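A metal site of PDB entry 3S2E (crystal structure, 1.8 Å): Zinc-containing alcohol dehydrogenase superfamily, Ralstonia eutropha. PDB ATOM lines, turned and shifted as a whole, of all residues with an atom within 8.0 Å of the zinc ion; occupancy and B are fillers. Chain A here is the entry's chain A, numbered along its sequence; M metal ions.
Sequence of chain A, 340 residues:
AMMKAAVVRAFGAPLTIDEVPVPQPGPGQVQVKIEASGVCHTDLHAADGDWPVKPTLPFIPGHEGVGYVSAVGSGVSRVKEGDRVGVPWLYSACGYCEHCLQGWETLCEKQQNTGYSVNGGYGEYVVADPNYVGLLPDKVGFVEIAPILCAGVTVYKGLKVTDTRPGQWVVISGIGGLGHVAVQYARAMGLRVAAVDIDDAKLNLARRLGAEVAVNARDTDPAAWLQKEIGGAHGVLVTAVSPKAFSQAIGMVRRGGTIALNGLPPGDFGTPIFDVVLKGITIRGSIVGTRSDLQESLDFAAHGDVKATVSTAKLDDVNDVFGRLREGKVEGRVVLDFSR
The backbone NH (N) of Gly 95 sits close to the side-chain sulfur (SG) of Cys 100.
SG of Cys 108 sits close to N of Lys 110 (3.4 Å).
The backbone NH of Tyr 96 sits close to the side-chain sulfur of Cys 94, 3.3 Å away.
SG of Cys 97 lies close to N of His 99, 3.5 Å away.
The side-chain amide nitrogen (NE2) of Gln 111 is in hydrogen-bond range of the backbone carbonyl oxygen (O) of Cys 108, at 2.9 Å.
Gly 95 touches the zinc ion.
Five residues have an atom within 4 Å of the zinc ion: Cys 94, Gly 95, Cys 97, Cys 100 and Cys 108.
The zinc ion is bound by the side-chain sulfur (SG) of Cys 94, the side-chain sulfur (SG) of Cys 108, the side-chain sulfur (SG) of Cys 100 and the side-chain sulfur (SG) of Cys 97.
The zinc ion has four donor atoms within binding distance.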
ATOM      1  N   SER A  92      33.170   9.949  15.388  1.00  0.00           N
ATOM      2  CA  SER A  92      32.813   8.736  16.093  1.00  0.00           C
ATOM      3  C   SER A  92      32.453   9.063  17.520  1.00  0.00           C
ATOM      4  O   SER A  92      32.819  10.122  18.033  1.00  0.00           O
ATOM      5  CB  SER A  92      33.989   7.720  16.082  1.00  0.00           C
ATOM      6  OG  SER A  92      35.121   8.231  16.799  1.00  0.00           O
ATOM      7  N   ALA A  93      31.713   8.147  18.152  1.00  0.00           N
ATOM      8  CA  ALA A  93      31.485   8.226  19.603  1.00  0.00           C
ATOM      9  C   ALA A  93      31.685   6.826  20.159  1.00  0.00           C
ATOM     10  O   ALA A  93      31.793   5.864  19.379  1.00  0.00           O
ATOM     11  CB  ALA A  93      30.069   8.771  19.913  1.00  0.00           C
ATOM     12  N   CYS A  94      31.747   6.716  21.494  1.00  0.00           N
ATOM     13  CA  CYS A  94      32.147   5.470  22.146  1.00  0.00           C
ATOM     14  C   CYS A  94      31.104   4.364  22.014  1.00  0.00           C
ATOM     15  O   CYS A  94      31.441   3.181  22.017  1.00  0.00           O
ATOM     16  CB  CYS A  94      32.488   5.715  23.636  1.00  0.00           C
ATOM     17  SG  CYS A  94      31.061   5.734  24.772  1.00  0.00           S
ATOM     18  N   GLY A  95      29.829   4.759  21.892  1.00  0.00           N
ATOM     19  CA  GLY A  95      28.725   3.840  21.683  1.00  0.00           C
ATOM     20  C   GLY A  95      28.117   3.222  22.947  1.00  0.00           C
ATOM     21  O   GLY A  95      27.068   2.585  22.858  1.00  0.00           O
ATOM     22  N   TYR A  96      28.745   3.423  24.096  1.00  0.00           N
ATOM     23  CA  TYR A  96      28.478   2.623  25.304  1.00  0.00           C
ATOM     24  C   TYR A  96      28.112   3.451  26.517  1.00  0.00           C
ATOM     25  O   TYR A  96      27.565   2.931  27.478  1.00  0.00           O
ATOM     26  CB  TYR A  96      29.710   1.775  25.678  1.00  0.00           C
ATOM     27  CG  TYR A  96      30.173   0.842  24.603  1.00  0.00           C
ATOM     28  CD1 TYR A  96      31.528   0.612  24.399  1.00  0.00           C
ATOM     29  CD2 TYR A  96      29.258   0.176  23.806  1.00  0.00           C
ATOM     30  CE1 TYR A  96      31.957  -0.266  23.405  1.00  0.00           C
ATOM     31  CE2 TYR A  96      29.665  -0.705  22.809  1.00  0.00           C
ATOM     32  CZ  TYR A  96      31.022  -0.920  22.614  1.00  0.00           C
ATOM     33  OH  TYR A  96      31.441  -1.782  21.617  1.00  0.00           O
ATOM     34  N   CYS A  97      28.446   4.730  26.476  1.00  0.00           N
ATOM     35  CA  CYS A  97      28.240   5.620  27.621  1.00  0.00           C
ATOM     36  C   CYS A  97      26.779   6.010  27.762  1.00  0.00           C
ATOM     37  O   CYS A  97      25.947   5.736  26.888  1.00  0.00           O
ATOM     38  CB  CYS A  97      29.136   6.860  27.502  1.00  0.00           C
ATOM     39  SG  CYS A  97      28.511   8.072  26.272  1.00  0.00           S
ATOM     40  N   GLU A  98      26.475   6.668  28.878  1.00  0.00           N
ATOM     41  CA  GLU A  98      25.102   7.052  29.198  1.00  0.00           C
ATOM     42  C   GLU A  98      24.479   7.821  28.014  1.00  0.00           C
ATOM     43  O   GLU A  98      23.323   7.613  27.647  1.00  0.00           O
ATOM     44  CB  GLU A  98      25.133   7.941  30.448  1.00  0.00           C
ATOM     45  CG  GLU A  98      23.823   8.630  30.797  1.00  0.00           C
ATOM     46  CD  GLU A  98      23.895   9.426  32.113  1.00  0.00           C
ATOM     47  OE1 GLU A  98      24.888  10.204  32.313  1.00  0.00           O
ATOM     48  OE2 GLU A  98      22.949   9.278  32.941  1.00  0.00           O
ATOM     49  N   HIS A  99      25.256   8.708  27.422  1.00  0.00           N
ATOM     50  CA  HIS A  99      24.762   9.538  26.328  1.00  0.00           C
ATOM     51  C   HIS A  99      24.539   8.750  25.035  1.00  0.00           C
ATOM     52  O   HIS A  99      23.499   8.867  24.387  1.00  0.00           O
ATOM     53  CB  HIS A  99      25.728  10.691  26.085  1.00  0.00           C
ATOM     54  CG  HIS A  99      25.974  11.536  27.286  1.00  0.00           C
ATOM     55  ND1 HIS A  99      24.948  12.094  28.023  1.00  0.00           N
ATOM     56  CD2 HIS A  99      27.120  11.916  27.893  1.00  0.00           C
ATOM     57  CE1 HIS A  99      25.458  12.789  29.029  1.00  0.00           C
ATOM     58  NE2 HIS A  99      26.778  12.697  28.972  1.00  0.00           N
ATOM     59  N   CYS A 100      25.536   7.958  24.658  1.00  0.00           N
ATOM     60  CA  CYS A 100      25.439   7.165  23.439  1.00  0.00           C
ATOM     61  C   CYS A 100      24.255   6.217  23.523  1.00  0.00           C
ATOM     62  O   CYS A 100      23.547   6.011  22.544  1.00  0.00           O
ATOM     63  CB  CYS A 100      26.721   6.369  23.185  1.00  0.00           C
ATOM     64  SG  CYS A 100      28.078   7.457  22.653  1.00  0.00           S
ATOM     65  N   LEU A 101      24.056   5.616  24.687  1.00  0.00           N
ATOM     66  CA  LEU A 101      22.978   4.644  24.803  1.00  0.00           C
ATOM     67  C   LEU A 101      21.610   5.316  24.683  1.00  0.00           C
ATOM     68  O   LEU A 101      20.638   4.705  24.239  1.00  0.00           O
ATOM     69  CB  LEU A 101      23.063   3.903  26.121  1.00  0.00           C
ATOM     70  CG  LEU A 101      24.187   2.877  26.286  1.00  0.00           C
ATOM     71  CD1 LEU A 101      24.021   2.188  27.626  1.00  0.00           C
ATOM     72  CD2 LEU A 101      24.216   1.868  25.148  1.00  0.00           C
ATOM     73  N   TRP A 104      22.141  10.207  22.207  1.00  0.00           N
ATOM     74  CA  TRP A 104      22.668  11.570  22.297  1.00  0.00           C
ATOM     75  C   TRP A 104      24.176  11.524  22.127  1.00  0.00           C
ATOM     76  O   TRP A 104      24.935  12.032  22.969  1.00  0.00           O
ATOM     77  CB  TRP A 104      22.315  12.197  23.661  1.00  0.00           C
ATOM     78  CG  TRP A 104      20.942  12.825  23.697  1.00  0.00           C
ATOM     79  CD1 TRP A 104      19.773  12.234  24.112  1.00  0.00           C
ATOM     80  CD2 TRP A 104      20.588  14.156  23.281  1.00  0.00           C
ATOM     81  NE1 TRP A 104      18.722  13.121  23.982  1.00  0.00           N
ATOM     82  CE2 TRP A 104      19.196  14.314  23.474  1.00  0.00           C
ATOM     83  CE3 TRP A 104      21.309  15.247  22.755  1.00  0.00           C
ATOM     84  CZ2 TRP A 104      18.513  15.501  23.173  1.00  0.00           C
ATOM     85  CZ3 TRP A 104      20.635  16.440  22.455  1.00  0.00           C
ATOM     86  CH2 TRP A 104      19.252  16.560  22.672  1.00  0.00           C
ATOM     87  N   GLU A 105      24.616  10.887  21.055  1.00  0.00           N
ATOM     88  CA  GLU A 105      26.040  10.678  20.862  1.00  0.00           C
ATOM     89  C   GLU A 105      26.811  12.004  20.723  1.00  0.00           C
ATOM     90  O   GLU A 105      28.025  12.017  20.872  1.00  0.00           O
ATOM     91  CB  GLU A 105      26.284   9.804  19.620  1.00  0.00           C
ATOM     92  CG  GLU A 105      25.654  10.340  18.351  1.00  0.00           C
ATOM     93  CD  GLU A 105      24.270   9.745  18.065  1.00  0.00           C
ATOM     94  OE1 GLU A 105      23.518   9.455  19.021  1.00  0.00           O
ATOM     95  OE2 GLU A 105      23.919   9.586  16.871  1.00  0.00           O
ATOM     96  N   THR A 106      26.097  13.105  20.444  1.00  0.00           N
ATOM     97  CA  THR A 106      26.762  14.414  20.369  1.00  0.00           C
ATOM     98  C   THR A 106      27.323  14.828  21.723  1.00  0.00           C
ATOM     99  O   THR A 106      28.193  15.696  21.792  1.00  0.00           O
ATOM    100  CB  THR A 106      25.817  15.556  19.922  1.00  0.00           C
ATOM    101  OG1 THR A 106      24.572  15.452  20.641  1.00  0.00           O
ATOM    102  CG2 THR A 106      25.563  15.458  18.425  1.00  0.00           C
ATOM    103  N   LEU A 107      26.809  14.239  22.777  1.00  0.00           N
ATOM    104  CA  LEU A 107      27.304  14.552  24.127  1.00  0.00           C
ATOM    105  C   LEU A 107      28.404  13.556  24.591  1.00  0.00           C
ATOM    106  O   LEU A 107      28.867  13.607  25.731  1.00  0.00           O
ATOM    107  CB  LEU A 107      26.137  14.549  25.118  1.00  0.00           C
ATOM    108  CG  LEU A 107      24.972  15.491  24.769  1.00  0.00           C
ATOM    109  CD1 LEU A 107      23.826  15.287  25.759  1.00  0.00           C
ATOM    110  CD2 LEU A 107      25.448  16.950  24.780  1.00  0.00           C
ATOM    111  N   CYS A 108      28.847  12.671  23.702  1.00  0.00           N
ATOM    112  CA  CYS A 108      29.836  11.671  24.125  1.00  0.00           C
ATOM    113  C   CYS A 108      31.164  12.320  24.499  1.00  0.00           C
ATOM    114  O   CYS A 108      31.768  12.983  23.669  1.00  0.00           O
ATOM    115  CB  CYS A 108      30.075  10.644  23.027  1.00  0.00           C
ATOM    116  SG  CYS A 108      31.235   9.333  23.578  1.00  0.00           S
ATOM    117  N   GLU A 109      31.627  12.090  25.723  1.00  0.00           N
ATOM    118  CA  GLU A 109      32.854  12.750  26.170  1.00  0.00           C
ATOM    119  C   GLU A 109      34.075  12.141  25.472  1.00  0.00           C
ATOM    120  O   GLU A 109      35.157  12.752  25.447  1.00  0.00           O
ATOM    121  CB  GLU A 109      32.962  12.680  27.694  1.00  0.00           C
ATOM    122  CG  GLU A 109      31.885  13.559  28.345  1.00  0.00           C
ATOM    123  CD  GLU A 109      31.914  13.536  29.871  1.00  0.00           C
ATOM    124  OE1 GLU A 109      31.033  14.193  30.474  1.00  0.00           O
ATOM    125  OE2 GLU A 109      32.810  12.876  30.444  1.00  0.00           O
ATOM    126  N   LYS A 110      33.897  10.969  24.891  1.00  0.00           N
ATOM    127  CA  LYS A 110      34.952  10.274  24.150  1.00  0.00           C
ATOM    128  C   LYS A 110      34.860  10.449  22.630  1.00  0.00           C
ATOM    129  O   LYS A 110      35.493   9.706  21.877  1.00  0.00           O
ATOM    130  CB  LYS A 110      34.947   8.775  24.472  1.00  0.00           C
ATOM    131  CG  LYS A 110      35.322   8.472  25.911  1.00  0.00           C
ATOM    132  CD  LYS A 110      35.590   7.001  26.118  1.00  0.00           C
ATOM    133  CE  LYS A 110      36.178   6.711  27.502  1.00  0.00           C
ATOM    134  NZ  LYS A 110      36.677   5.313  27.603  1.00  0.00           N
ATOM    135  N   GLN A 111      34.078  11.414  22.166  1.00  0.00           N
ATOM    136  CA  GLN A 111      33.907  11.567  20.726  1.00  0.00           C
ATOM    137  C   GLN A 111      35.188  12.035  20.055  1.00  0.00           C
ATOM    138  O   GLN A 111      36.026  12.706  20.685  1.00  0.00           O
ATOM    139  CB  GLN A 111      32.766  12.541  20.399  1.00  0.00           C
ATOM    140  CG  GLN A 111      33.113  14.002  20.652  1.00  0.00           C
ATOM    141  CD  GLN A 111      31.897  14.900  20.542  1.00  0.00           C
ATOM    142  OE1 GLN A 111      31.705  15.613  19.543  1.00  0.00           O
ATOM    143  NE2 GLN A 111      31.045  14.846  21.564  1.00  0.00           N
ATOM    144  N   TYR A 132      29.016   6.487  11.492  1.00  0.00           N
ATOM    145  CA  TYR A 132      28.772   7.901  11.834  1.00  0.00           C
ATOM    146  C   TYR A 132      28.736   8.824  10.622  1.00  0.00           C
ATOM    147  O   TYR A 132      28.478  10.022  10.755  1.00  0.00           O
ATOM    148  CB  TYR A 132      29.815   8.393  12.862  1.00  0.00           C
ATOM    149  CG  TYR A 132      29.612   7.706  14.205  1.00  0.00           C
ATOM    150  CD1 TYR A 132      30.195   6.461  14.462  1.00  0.00           C
ATOM    151  CD2 TYR A 132      28.789   8.254  15.174  1.00  0.00           C
ATOM    152  CE1 TYR A 132      29.968   5.803  15.666  1.00  0.00           C
ATOM    153  CE2 TYR A 132      28.570   7.602  16.379  1.00  0.00           C
ATOM    154  CZ  TYR A 132      29.163   6.382  16.615  1.00  0.00           C
ATOM    155  OH  TYR A 132      28.944   5.730  17.820  1.00  0.00           O
HETATM  156 ZN    ZN M   1      29.761   7.641  24.301  1.00  0.00          ZN
